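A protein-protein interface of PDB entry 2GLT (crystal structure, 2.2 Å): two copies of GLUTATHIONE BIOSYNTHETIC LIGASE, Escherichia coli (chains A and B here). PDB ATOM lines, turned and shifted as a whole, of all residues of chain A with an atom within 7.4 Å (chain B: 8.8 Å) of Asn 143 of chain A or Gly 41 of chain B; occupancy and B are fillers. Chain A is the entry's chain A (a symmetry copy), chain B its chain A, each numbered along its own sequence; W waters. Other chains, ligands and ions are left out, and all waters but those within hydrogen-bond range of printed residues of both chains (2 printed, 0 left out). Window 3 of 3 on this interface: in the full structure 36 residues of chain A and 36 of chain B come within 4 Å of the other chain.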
ATOM      1  N   LEU A 139     -11.367  -0.749   8.147  1.00  0.00           N
ATOM      2  CA  LEU A 139     -12.635  -0.285   8.677  1.00  0.00           C
ATOM      3  C   LEU A 139     -12.355   0.765   9.738  1.00  0.00           C
ATOM      4  O   LEU A 139     -11.549   0.525  10.639  1.00  0.00           O
ATOM      5  CB  LEU A 139     -13.386  -1.474   9.278  1.00  0.00           C
ATOM      6  CG  LEU A 139     -14.616  -1.255  10.137  1.00  0.00           C
ATOM      7  CD1 LEU A 139     -15.713  -0.556   9.353  1.00  0.00           C
ATOM      8  CD2 LEU A 139     -15.069  -2.596  10.662  1.00  0.00           C
ATOM      9  N   VAL A 140     -12.920   1.974   9.656  1.00  0.00           N
ATOM     10  CA  VAL A 140     -12.834   2.969  10.741  1.00  0.00           C
ATOM     11  C   VAL A 140     -14.218   3.006  11.411  1.00  0.00           C
ATOM     12  O   VAL A 140     -15.181   3.301  10.708  1.00  0.00           O
ATOM     13  CB  VAL A 140     -12.483   4.340  10.171  1.00  0.00           C
ATOM     14  CG1 VAL A 140     -12.448   5.393  11.292  1.00  0.00           C
ATOM     15  CG2 VAL A 140     -11.107   4.244   9.506  1.00  0.00           C
ATOM     16  N   THR A 141     -14.389   2.695  12.713  1.00  0.00           N
ATOM     17  CA  THR A 141     -15.705   2.571  13.358  1.00  0.00           C
ATOM     18  C   THR A 141     -15.656   2.714  14.875  1.00  0.00           C
ATOM     19  O   THR A 141     -14.609   2.525  15.495  1.00  0.00           O
ATOM     20  CB  THR A 141     -16.343   1.172  13.011  1.00  0.00           C
ATOM     21  OG1 THR A 141     -17.710   1.182  13.432  1.00  0.00           O
ATOM     22  CG2 THR A 141     -15.634   0.013  13.721  1.00  0.00           C
ATOM     23  N   ARG A 142     -16.820   2.924  15.495  1.00  0.00           N
ATOM     24  CA  ARG A 142     -16.935   3.028  16.936  1.00  0.00           C
ATOM     25  C   ARG A 142     -17.547   1.782  17.546  1.00  0.00           C
ATOM     26  O   ARG A 142     -17.579   1.592  18.762  1.00  0.00           O
ATOM     27  CB  ARG A 142     -17.813   4.211  17.333  1.00  0.00           C
ATOM     28  CG  ARG A 142     -17.123   5.547  17.101  1.00  0.00           C
ATOM     29  CD  ARG A 142     -17.808   6.706  17.812  1.00  0.00           C
ATOM     30  NE  ARG A 142     -17.053   7.941  17.636  1.00  0.00           N
ATOM     31  CZ  ARG A 142     -17.460   9.108  18.172  1.00  0.00           C
ATOM     32  NH1 ARG A 142     -18.580   9.185  18.884  1.00  0.00           N
ATOM     33  NH2 ARG A 142     -16.714  10.212  18.047  1.00  0.00           N
ATOM     34  N   ASN A 143     -18.077   0.877  16.731  1.00  0.00           N
ATOM     35  CA  ASN A 143     -18.682  -0.306  17.320  1.00  0.00           C
ATOM     36  C   ASN A 143     -18.191  -1.707  17.043  1.00  0.00           C
ATOM     37  O   ASN A 143     -17.748  -2.086  15.970  1.00  0.00           O
ATOM     38  CB  ASN A 143     -20.166  -0.300  17.059  1.00  0.00           C
ATOM     39  CG  ASN A 143     -20.652   0.308  15.778  1.00  0.00           C
ATOM     40  OD1 ASN A 143     -20.832   1.518  15.661  1.00  0.00           O
ATOM     41  ND2 ASN A 143     -20.946  -0.568  14.832  1.00  0.00           N
ATOM     42  N   LYS A 144     -18.307  -2.383  18.182  1.00  0.00           N
ATOM     43  CA  LYS A 144     -17.903  -3.737  18.428  1.00  0.00           C
ATOM     44  C   LYS A 144     -18.418  -4.720  17.397  1.00  0.00           C
ATOM     45  O   LYS A 144     -17.638  -5.431  16.764  1.00  0.00           O
ATOM     46  CB  LYS A 144     -18.378  -4.102  19.839  1.00  0.00           C
ATOM     47  CG  LYS A 144     -17.644  -5.318  20.452  1.00  0.00           C
ATOM     48  CD  LYS A 144     -18.209  -5.848  21.777  1.00  0.00           C
ATOM     49  CE  LYS A 144     -18.203  -4.863  22.941  1.00  0.00           C
ATOM     50  NZ  LYS A 144     -16.848  -4.445  23.244  1.00  0.00           N
ATOM     51  N   ALA A 145     -19.731  -4.728  17.170  1.00  0.00           N
ATOM     52  CA  ALA A 145     -20.334  -5.623  16.202  1.00  0.00           C
ATOM     53  C   ALA A 145     -19.776  -5.499  14.789  1.00  0.00           C
ATOM     54  O   ALA A 145     -19.685  -6.481  14.060  1.00  0.00           O
ATOM     55  CB  ALA A 145     -21.828  -5.369  16.178  1.00  0.00           C
ATOM     56  N   GLN A 146     -19.349  -4.313  14.367  1.00  0.00           N
ATOM     57  CA  GLN A 146     -18.770  -4.148  13.050  1.00  0.00           C
ATOM     58  C   GLN A 146     -17.350  -4.672  13.040  1.00  0.00           C
ATOM     59  O   GLN A 146     -16.953  -5.297  12.058  1.00  0.00           O
ATOM     60  CB  GLN A 146     -18.776  -2.693  12.656  1.00  0.00           C
ATOM     61  CG  GLN A 146     -20.144  -2.371  12.104  1.00  0.00           C
ATOM     62  CD  GLN A 146     -20.254  -0.998  11.483  1.00  0.00           C
ATOM     63  OE1 GLN A 146     -20.498  -0.005  12.146  1.00  0.00           O
ATOM     64  NE2 GLN A 146     -20.080  -0.855  10.187  1.00  0.00           N
ATOM     65  N   LEU A 147     -16.614  -4.490  14.148  1.00  0.00           N
ATOM     66  CA  LEU A 147     -15.252  -4.980  14.258  1.00  0.00           C
ATOM     67  C   LEU A 147     -15.199  -6.512  14.263  1.00  0.00           C
ATOM     68  O   LEU A 147     -14.378  -7.123  13.588  1.00  0.00           O
ATOM     69  CB  LEU A 147     -14.638  -4.395  15.527  1.00  0.00           C
ATOM     70  CG  LEU A 147     -14.386  -2.885  15.567  1.00  0.00           C
ATOM     71  CD1 LEU A 147     -13.855  -2.509  16.912  1.00  0.00           C
ATOM     72  CD2 LEU A 147     -13.368  -2.481  14.546  1.00  0.00           C
ATOM     73  N   LYS A 148     -16.137  -7.114  14.995  1.00  0.00           N
ATOM     74  CA  LYS A 148     -16.327  -8.559  15.139  1.00  0.00           C
ATOM     75  C   LYS A 148     -16.626  -9.166  13.789  1.00  0.00           C
ATOM     76  O   LYS A 148     -16.053 -10.184  13.419  1.00  0.00           O
ATOM     77  CB  LYS A 148     -17.489  -8.848  16.072  1.00  0.00           C
ATOM     78  CG  LYS A 148     -17.588 -10.309  16.415  1.00  0.00           C
ATOM     79  CD  LYS A 148     -18.838 -10.716  17.194  1.00  0.00           C
ATOM     80  CE  LYS A 148     -18.585 -12.177  17.637  1.00  0.00           C
ATOM     81  NZ  LYS A 148     -19.674 -12.801  18.382  1.00  0.00           N
ATOM     82  N   ALA A 149     -17.484  -8.472  13.046  1.00  0.00           N
ATOM     83  CA  ALA A 149     -17.843  -8.846  11.699  1.00  0.00           C
ATOM     84  C   ALA A 149     -16.723  -8.730  10.694  1.00  0.00           C
ATOM     85  O   ALA A 149     -16.637  -9.514   9.744  1.00  0.00           O
ATOM     86  CB  ALA A 149     -18.954  -7.980  11.209  1.00  0.00           C
ATOM     87  N   ALA A 184     -11.812  -4.018  21.739  1.00  0.00           N
ATOM     88  CA  ALA A 184     -12.614  -3.056  21.019  1.00  0.00           C
ATOM     89  C   ALA A 184     -13.236  -2.079  22.008  1.00  0.00           C
ATOM     90  O   ALA A 184     -13.360  -0.893  21.692  1.00  0.00           O
ATOM     91  CB  ALA A 184     -13.706  -3.780  20.240  1.00  0.00           C
ATOM     92  N   GLU A 185     -13.543  -2.539  23.227  1.00  0.00           N
ATOM     93  CA  GLU A 185     -14.060  -1.679  24.261  1.00  0.00           C
ATOM     94  C   GLU A 185     -13.023  -0.739  24.852  1.00  0.00           C
ATOM     95  O   GLU A 185     -13.347   0.387  25.235  1.00  0.00           O
ATOM     96  CB  GLU A 185     -14.681  -2.556  25.335  1.00  0.00           C
ATOM     97  CG  GLU A 185     -16.019  -1.953  25.828  1.00  0.00           C
ATOM     98  CD  GLU A 185     -17.145  -1.495  24.843  1.00  0.00           C
ATOM     99  OE1 GLU A 185     -16.992  -1.516  23.613  1.00  0.00           O
ATOM    100  OE2 GLU A 185     -18.220  -1.081  25.308  1.00  0.00           O
ATOM    101  N   THR A 188     -12.066   1.723  21.594  1.00  0.00           N
ATOM    102  CA  THR A 188     -13.131   2.660  21.292  1.00  0.00           C
ATOM    103  C   THR A 188     -13.562   3.409  22.545  1.00  0.00           C
ATOM    104  O   THR A 188     -14.495   4.194  22.470  1.00  0.00           O
ATOM    105  CB  THR A 188     -14.372   1.951  20.715  1.00  0.00           C
ATOM    106  OG1 THR A 188     -14.880   1.115  21.746  1.00  0.00           O
ATOM    107  CG2 THR A 188     -14.080   1.236  19.438  1.00  0.00           C
ATOM    108  N   GLY A 191     -17.218   2.566  22.926  1.00  0.00           N
ATOM    109  CA  GLY A 191     -18.054   3.000  21.832  1.00  0.00           C
ATOM    110  C   GLY A 191     -18.096   4.498  21.618  1.00  0.00           C
ATOM    111  O   GLY A 191     -18.981   4.963  20.906  1.00  0.00           O
ATOM    112  N   THR A 192     -17.151   5.257  22.179  1.00  0.00           N
ATOM    113  CA  THR A 192     -17.163   6.709  22.098  1.00  0.00           C
ATOM    114  C   THR A 192     -16.094   7.275  21.208  1.00  0.00           C
ATOM    115  O   THR A 192     -16.113   8.488  20.963  1.00  0.00           O
ATOM    116  CB  THR A 192     -17.010   7.339  23.509  1.00  0.00           C
ATOM    117  OG1 THR A 192     -15.790   6.873  24.045  1.00  0.00           O
ATOM    118  CG2 THR A 192     -18.128   6.962  24.463  1.00  0.00           C
ATOM    119  N   ARG A 193     -15.151   6.438  20.732  1.00  0.00           N
ATOM    120  CA  ARG A 193     -14.056   6.889  19.871  1.00  0.00           C
ATOM    121  C   ARG A 193     -13.867   5.985  18.686  1.00  0.00           C
ATOM    122  O   ARG A 193     -14.014   4.780  18.826  1.00  0.00           O
ATOM    123  CB  ARG A 193     -12.708   6.925  20.601  1.00  0.00           C
ATOM    124  CG  ARG A 193     -12.752   7.893  21.770  1.00  0.00           C
ATOM    125  CD  ARG A 193     -11.438   8.018  22.481  1.00  0.00           C
ATOM    126  NE  ARG A 193     -10.556   9.002  21.880  1.00  0.00           N
ATOM    127  CZ  ARG A 193     -10.730  10.324  22.035  1.00  0.00           C
ATOM    128  NH1 ARG A 193     -11.729  10.850  22.762  1.00  0.00           N
ATOM    129  NH2 ARG A 193      -9.855  11.141  21.450  1.00  0.00           N
ATOM    130  N   TYR A 194     -13.545   6.527  17.514  1.00  0.00           N
ATOM    131  CA  TYR A 194     -13.283   5.736  16.334  1.00  0.00           C
ATOM    132  C   TYR A 194     -11.953   5.005  16.518  1.00  0.00           C
ATOM    133  O   TYR A 194     -11.031   5.482  17.173  1.00  0.00           O
ATOM    134  CB  TYR A 194     -13.171   6.607  15.078  1.00  0.00           C
ATOM    135  CG  TYR A 194     -14.415   7.405  14.708  1.00  0.00           C
ATOM    136  CD1 TYR A 194     -15.548   6.746  14.213  1.00  0.00           C
ATOM    137  CD2 TYR A 194     -14.446   8.783  14.922  1.00  0.00           C
ATOM    138  CE1 TYR A 194     -16.725   7.451  13.979  1.00  0.00           C
ATOM    139  CE2 TYR A 194     -15.615   9.496  14.681  1.00  0.00           C
ATOM    140  CZ  TYR A 194     -16.748   8.816  14.231  1.00  0.00           C
ATOM    141  OH  TYR A 194     -17.927   9.487  14.041  1.00  0.00           O
ATOM    142  N   CYS A 195     -11.901   3.774  16.012  1.00  0.00           N
ATOM    143  CA  CYS A 195     -10.681   2.996  15.938  1.00  0.00           C
ATOM    144  C   CYS A 195     -10.599   2.458  14.509  1.00  0.00           C
ATOM    145  O   CYS A 195     -11.542   2.613  13.728  1.00  0.00           O
ATOM    146  CB  CYS A 195     -10.694   1.836  16.955  1.00  0.00           C
ATOM    147  SG  CYS A 195     -11.670   0.308  16.803  1.00  0.00           S
ATOM    148  N   VAL B   7     -26.468  14.756  11.273  1.00  0.00           N
ATOM    149  CA  VAL B   7     -25.632  14.208  12.334  1.00  0.00           C
ATOM    150  C   VAL B   7     -25.729  15.165  13.507  1.00  0.00           C
ATOM    151  O   VAL B   7     -25.370  16.343  13.436  1.00  0.00           O
ATOM    152  CB  VAL B   7     -24.150  14.073  11.931  1.00  0.00           C
ATOM    153  CG1 VAL B   7     -23.437  13.326  13.065  1.00  0.00           C
ATOM    154  CG2 VAL B   7     -23.976  13.225  10.702  1.00  0.00           C
ATOM    155  N   MET B   8     -26.224  14.643  14.613  1.00  0.00           N
ATOM    156  CA  MET B   8     -26.479  15.466  15.774  1.00  0.00           C
ATOM    157  C   MET B   8     -26.362  14.645  17.047  1.00  0.00           C
ATOM    158  O   MET B   8     -26.162  13.440  17.055  1.00  0.00           O
ATOM    159  CB  MET B   8     -27.904  16.116  15.620  1.00  0.00           C
ATOM    160  CG  MET B   8     -29.099  15.147  15.527  1.00  0.00           C
ATOM    161  SD  MET B   8     -30.701  15.826  16.041  1.00  0.00           S
ATOM    162  CE  MET B   8     -31.285  15.980  14.423  1.00  0.00           C
ATOM    163  N   MET B  38     -28.731  10.436  12.113  1.00  0.00           N
ATOM    164  CA  MET B  38     -27.470   9.802  12.471  1.00  0.00           C
ATOM    165  C   MET B  38     -26.860  10.444  13.690  1.00  0.00           C
ATOM    166  O   MET B  38     -26.966  11.648  13.886  1.00  0.00           O
ATOM    167  CB  MET B  38     -26.363   9.918  11.380  1.00  0.00           C
ATOM    168  CG  MET B  38     -26.676   9.211  10.063  1.00  0.00           C
ATOM    169  SD  MET B  38     -25.731   9.823   8.664  1.00  0.00           S
ATOM    170  CE  MET B  38     -26.645  11.290   8.296  1.00  0.00           C
ATOM    171  N   GLU B  39     -26.240   9.628  14.552  1.00  0.00           N
ATOM    172  CA  GLU B  39     -25.371  10.107  15.619  1.00  0.00           C
ATOM    173  C   GLU B  39     -23.937   9.800  15.150  1.00  0.00           C
ATOM    174  O   GLU B  39     -23.674   9.104  14.157  1.00  0.00           O
ATOM    175  CB  GLU B  39     -25.692   9.399  16.906  1.00  0.00           C
ATOM    176  CG  GLU B  39     -27.087   9.783  17.414  1.00  0.00           C
ATOM    177  CD  GLU B  39     -27.602   9.148  18.702  1.00  0.00           C
ATOM    178  OE1 GLU B  39     -26.791   8.722  19.524  1.00  0.00           O
ATOM    179  OE2 GLU B  39     -28.821   9.087  18.911  1.00  0.00           O
ATOM    180  N   MET B  40     -22.964  10.377  15.838  1.00  0.00           N
ATOM    181  CA  MET B  40     -21.558  10.185  15.536  1.00  0.00           C
ATOM    182  C   MET B  40     -21.100   8.746  15.340  1.00  0.00           C
ATOM    183  O   MET B  40     -20.461   8.421  14.351  1.00  0.00           O
ATOM    184  CB  MET B  40     -20.767  10.808  16.642  1.00  0.00           C
ATOM    185  CG  MET B  40     -20.781  12.303  16.577  1.00  0.00           C
ATOM    186  SD  MET B  40     -19.652  12.913  15.321  1.00  0.00           S
ATOM    187  CE  MET B  40     -18.398  13.566  16.386  1.00  0.00           C
ATOM    188  N   GLY B  41     -21.448   7.865  16.256  1.00  0.00           N
ATOM    189  CA  GLY B  41     -21.096   6.463  16.172  1.00  0.00           C
ATOM    190  C   GLY B  41     -21.764   5.703  15.024  1.00  0.00           C
ATOM    191  O   GLY B  41     -21.419   4.541  14.815  1.00  0.00           O
ATOM    192  N   ASP B  42     -22.721   6.285  14.282  1.00  0.00           N
ATOM    193  CA  ASP B  42     -23.337   5.602  13.160  1.00  0.00           C
ATOM    194  C   ASP B  42     -22.533   5.727  11.877  1.00  0.00           C
ATOM    195  O   ASP B  42     -22.790   5.006  10.906  1.00  0.00           O
ATOM    196  CB  ASP B  42     -24.792   6.146  12.928  1.00  0.00           C
ATOM    197  CG  ASP B  42     -25.750   5.712  14.041  1.00  0.00           C
ATOM    198  OD1 ASP B  42     -25.784   4.537  14.402  1.00  0.00           O
ATOM    199  OD2 ASP B  42     -26.447   6.546  14.603  1.00  0.00           O
ATOM    200  N   LEU B  43     -21.562   6.655  11.859  1.00  0.00           N
ATOM    201  CA  LEU B  43     -20.734   6.958  10.711  1.00  0.00           C
ATOM    202  C   LEU B  43     -19.564   6.019  10.675  1.00  0.00           C
ATOM    203  O   LEU B  43     -19.004   5.778  11.750  1.00  0.00           O
ATOM    204  CB  LEU B  43     -20.197   8.362  10.812  1.00  0.00           C
ATOM    205  CG  LEU B  43     -21.149   9.535  10.907  1.00  0.00           C
ATOM    206  CD1 LEU B  43     -20.297  10.778  11.029  1.00  0.00           C
ATOM    207  CD2 LEU B  43     -22.021   9.665   9.682  1.00  0.00           C
ATOM    208  N   TYR B  44     -19.198   5.460   9.512  1.00  0.00           N
ATOM    209  CA  TYR B  44     -18.006   4.642   9.411  1.00  0.00           C
ATOM    210  C   TYR B  44     -17.449   4.649   7.998  1.00  0.00           C
ATOM    211  O   TYR B  44     -18.061   5.170   7.068  1.00  0.00           O
ATOM    212  CB  TYR B  44     -18.282   3.201   9.876  1.00  0.00           C
ATOM    213  CG  TYR B  44     -19.150   2.353   8.970  1.00  0.00           C
ATOM    214  CD1 TYR B  44     -20.533   2.400   9.107  1.00  0.00           C
ATOM    215  CD2 TYR B  44     -18.547   1.514   8.013  1.00  0.00           C
ATOM    216  CE1 TYR B  44     -21.325   1.597   8.299  1.00  0.00           C
ATOM    217  CE2 TYR B  44     -19.342   0.714   7.207  1.00  0.00           C
ATOM    218  CZ  TYR B  44     -20.725   0.755   7.357  1.00  0.00           C
ATOM    219  OH  TYR B  44     -21.512  -0.049   6.560  1.00  0.00           O
ATOM    220  N   LEU B  45     -16.264   4.076   7.777  1.00  0.00           N
ATOM    221  CA  LEU B  45     -15.583   4.184   6.493  1.00  0.00           C
ATOM    222  C   LEU B  45     -15.138   2.787   6.193  1.00  0.00           C
ATOM    223  O   LEU B  45     -14.474   2.164   7.017  1.00  0.00           O
ATOM    224  CB  LEU B  45     -14.406   5.099   6.679  1.00  0.00           C
ATOM    225  CG  LEU B  45     -13.835   5.905   5.558  1.00  0.00           C
ATOM    226  CD1 LEU B  45     -14.778   7.010   5.159  1.00  0.00           C
ATOM    227  CD2 LEU B  45     -12.559   6.561   6.055  1.00  0.00           C
ATOM    228  N   ARG B  51     -20.034   5.535   4.902  1.00  0.00           N
ATOM    229  CA  ARG B  51     -21.329   4.913   5.104  1.00  0.00           C
ATOM    230  C   ARG B  51     -21.829   5.198   6.503  1.00  0.00           C
ATOM    231  O   ARG B  51     -21.127   5.650   7.423  1.00  0.00           O
ATOM    232  CB  ARG B  51     -21.268   3.390   4.971  1.00  0.00           C
ATOM    233  CG  ARG B  51     -20.716   2.788   3.671  1.00  0.00           C
ATOM    234  CD  ARG B  51     -21.218   1.340   3.695  1.00  0.00           C
ATOM    235  NE  ARG B  51     -21.594   1.081   2.348  1.00  0.00           N
ATOM    236  CZ  ARG B  51     -22.786   0.626   2.007  1.00  0.00           C
ATOM    237  NH1 ARG B  51     -23.755   0.348   2.878  1.00  0.00           N
ATOM    238  NH2 ARG B  51     -23.002   0.511   0.718  1.00  0.00           N
ATOM    239  N   ALA B  52     -23.100   4.895   6.675  1.00  0.00           N
ATOM    240  CA  ALA B  52     -23.686   5.056   7.974  1.00  0.00           C
ATOM    241  C   ALA B  52     -24.937   4.245   8.100  1.00  0.00           C
ATOM    242  O   ALA B  52     -25.592   3.890   7.127  1.00  0.00           O
ATOM    243  CB  ALA B  52     -24.057   6.516   8.233  1.00  0.00           C
ATOM    244  N   HIS B  53     -25.226   3.951   9.348  1.00  0.00           N
ATOM    245  CA  HIS B  53     -26.484   3.380   9.749  1.00  0.00           C
ATOM    246  C   HIS B  53     -27.447   4.564   9.980  1.00  0.00           C
ATOM    247  O   HIS B  53     -27.228   5.391  10.882  1.00  0.00           O
ATOM    248  CB  HIS B  53     -26.232   2.590  11.019  1.00  0.00           C
ATOM    249  CG  HIS B  53     -27.476   2.306  11.830  1.00  0.00           C
ATOM    250  ND1 HIS B  53     -27.888   2.970  12.914  1.00  0.00           N
ATOM    251  CD2 HIS B  53     -28.395   1.339  11.532  1.00  0.00           C
ATOM    252  CE1 HIS B  53     -29.016   2.454  13.283  1.00  0.00           C
ATOM    253  NE2 HIS B  53     -29.305   1.479  12.447  1.00  0.00           N
ATOM    254  N   ASP B  74     -28.591   0.653   6.338  1.00  0.00           N
ATOM    255  CA  ASP B  74     -27.181   0.928   6.253  1.00  0.00           C
ATOM    256  C   ASP B  74     -26.922   1.437   4.848  1.00  0.00           C
ATOM    257  O   ASP B  74     -26.954   0.618   3.943  1.00  0.00           O
ATOM    258  CB  ASP B  74     -26.465  -0.359   6.520  1.00  0.00           C
ATOM    259  CG  ASP B  74     -24.960  -0.232   6.400  1.00  0.00           C
ATOM    260  OD1 ASP B  74     -24.329   0.159   7.381  1.00  0.00           O
ATOM    261  OD2 ASP B  74     -24.422  -0.540   5.337  1.00  0.00           O
ATOM    262  N   LYS B  87     -23.585  18.486  14.993  1.00  0.00           N
ATOM    263  CA  LYS B  87     -22.953  17.985  16.208  1.00  0.00           C
ATOM    264  C   LYS B  87     -22.466  19.134  17.102  1.00  0.00           C
ATOM    265  O   LYS B  87     -21.878  20.107  16.647  1.00  0.00           O
ATOM    266  CB  LYS B  87     -21.777  17.094  15.804  1.00  0.00           C
ATOM    267  CG  LYS B  87     -20.984  16.487  16.943  1.00  0.00           C
ATOM    268  CD  LYS B  87     -21.937  15.617  17.733  1.00  0.00           C
ATOM    269  CE  LYS B  87     -21.199  15.067  18.932  1.00  0.00           C
ATOM    270  NZ  LYS B  87     -20.793  16.086  19.883  1.00  0.00           N
ATOM    271  N   GLU B  94     -12.054  13.793  17.832  1.00  0.00           N
ATOM    272  CA  GLU B  94     -13.164  12.994  17.354  1.00  0.00           C
ATOM    273  C   GLU B  94     -14.050  13.654  16.303  1.00  0.00           C
ATOM    274  O   GLU B  94     -14.538  13.001  15.360  1.00  0.00           O
ATOM    275  CB  GLU B  94     -14.060  12.563  18.500  1.00  0.00           C
ATOM    276  CG  GLU B  94     -13.517  11.387  19.286  1.00  0.00           C
ATOM    277  CD  GLU B  94     -13.054  10.189  18.451  1.00  0.00           C
ATOM    278  OE1 GLU B  94     -13.873   9.579  17.766  1.00  0.00           O
ATOM    279  OE2 GLU B  94     -11.865   9.876  18.508  1.00  0.00           O
ATOM    280  N   ALA B  98     -14.578  12.728  12.175  1.00  0.00           N
ATOM    281  CA  ALA B  98     -15.879  12.686  11.505  1.00  0.00           C
ATOM    282  C   ALA B  98     -15.986  13.553  10.275  1.00  0.00           C
ATOM    283  O   ALA B  98     -16.676  13.278   9.300  1.00  0.00           O
ATOM    284  CB  ALA B  98     -16.952  13.102  12.469  1.00  0.00           C
ATOM    285  N   ILE B 101     -14.736  11.606   7.218  1.00  0.00           N
ATOM    286  CA  ILE B 101     -15.769  10.667   6.727  1.00  0.00           C
ATOM    287  C   ILE B 101     -16.801  11.419   5.874  1.00  0.00           C
ATOM    288  O   ILE B 101     -17.124  11.011   4.748  1.00  0.00           O
ATOM    289  CB  ILE B 101     -16.443   9.959   7.942  1.00  0.00           C
ATOM    290  CG1 ILE B 101     -15.370   9.111   8.589  1.00  0.00           C
ATOM    291  CG2 ILE B 101     -17.638   9.070   7.548  1.00  0.00           C
ATOM    292  CD1 ILE B 101     -15.791   8.501   9.937  1.00  0.00           C
HETATM  293  O   HOH W   1     -23.030   1.955  12.398  1.00  0.00           O
HETATM  294  O   HOH W   2     -18.752   4.191  13.984  1.00  0.00           O
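OH of Tyr 194 of chain A is in hydrogen-bond range of O of Met 40 of chain B. OD1 of Asn 143 of chain A lies close to O of Gly 41 of chain B, 3.2 Å away. The backbone carbonyl oxygen (O) of Leu 45 of chain B sits at hydrogen-bond distance from the backbone NH (N) of Val 140 of chain A (3.1 Å). The side-chain carboxylate of Glu 94 of chain B is in salt-bridge range of the guanidinium group of Arg 142 of chain A, at 2.9 Å. The side-chain carboxylate (OE2) of Glu 94 of chain B lies within salt-bridge range of the guanidinium group (NE) of Arg 193 of chain A. N of Tyr 194 of chain A lies close to OE1 of Glu 94 of chain B (3.1 Å).
The backbone NH (N) of Tyr 44 of chain B is in hydrogen-bond range of the backbone carbonyl oxygen (O) of Arg 51 of chain B (2.8 Å). OH of Tyr 44 of chain B sits at hydrogen-bond distance from OD1 of Asp 74 of chain B, at 2.9 Å. The side-chain hydroxyl (OG1) of Thr 141 of chain A is in hydrogen-bond range of the backbone NH (N) of Asn 143 of chain A (3.3 Å). OE1 of Gln 146 of chain A lies within hydrogen-bond range of OG1 of Thr 141 of chain A (3.3 Å). The guanidinium group (NH1) of Arg 142 of chain A lies close to the backbone carbonyl oxygen (O) of Thr 192 of chain A (3.3 Å). The backbone carbonyl oxygen of Thr 188 of chain A sits at hydrogen-bond distance from the backbone NH of Arg 193 of chain A (2.9 Å).
Tyr 44 of chain B touches Leu 139 of chain A. Leu 45 of chain B touches Leu 139 of chain A (O to CA, 3.5 Å). Val 140 of chain A touches Tyr 44 of chain B (O to CB, 3.2 Å). CB of Met 40 of chain B touches NH1 of Arg 142 of chain A, at 3.5 Å. CD of Arg 142 of chain A touches CA of Gly 41 of chain B, at 3.7 Å. Gln 146 of chain A touches Tyr 44 of chain B (NE2 to CZ, 3.3 Å). Leu 43 of chain B touches Tyr 194 of chain A.
Of the printed residues of chain B, Leu 139 of chain A touches Tyr 44 and Leu 45. Printed residues of chain B within 4 Å of Val 140 of chain A: Tyr 44 and Leu 45. Of the printed residues of chain B, Arg 193 of chain A touches Glu 94 (3.4 Å). Met 8 of chain B touches none of the printed residues of chain A. Gly 41 of chain B touches just these residues of chain A: Arg 142 (3.7 Å) and Asn 143 (3.2 Å). Lys 87 of chain B touches none of the printed residues of chain A. The nearest residue of chain B that does not touch Asn 143 of chain A is Asp 42 of chain B (5.3 Å). The nearest residue of chain A that does not touch Gly 41 of chain B is Tyr 194 of chain A (4.5 Å). The nearest printed residue of chain B that does not touch Gln 146 of chain A is Asp 74 of chain B (5.2 Å).
Of the 18 printed residues of chain B, 6 touch a printed residue of chain A. Along chain B the printed residues that touch a printed residue of chain A span positions 40 to 94. Printed residues of chain A that touch a printed residue of chain B: Leu 139, Val 140, Arg 142, Asn 143, Gln 146, Arg 193 and Tyr 194. Hydrophobic or aromatic side chains of chain A within 4 Å of the printed part of chain B: Leu 139 and Tyr 194. Among the printed residues, Asp or Glu carboxylates within 4 Å of a Lys or Arg side-chain nitrogen of the other chain: Arg 142 of chain A with Glu 94 of chain B and Arg 193 of chain A with Glu 94 of chain B.
No position is printed for both chains.
Water W2 lies within hydrogen-bond range of the backbone carbonyl oxygen of Leu 43 of chain B (2.8 Å), the backbone NH of Arg 142 of chain A (2.8 Å), the backbone carbonyl oxygen of Gly 41 of chain B (2.8 Å) and the side-chain hydroxyl of Thr 141 of chain A (3.2 Å). Water W1 lies within hydrogen-bond range of the side-chain amide oxygen of Gln 146 of chain A (3.2 Å) and the backbone carbonyl oxygen of Asp 42 of chain B (3.4 Å).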
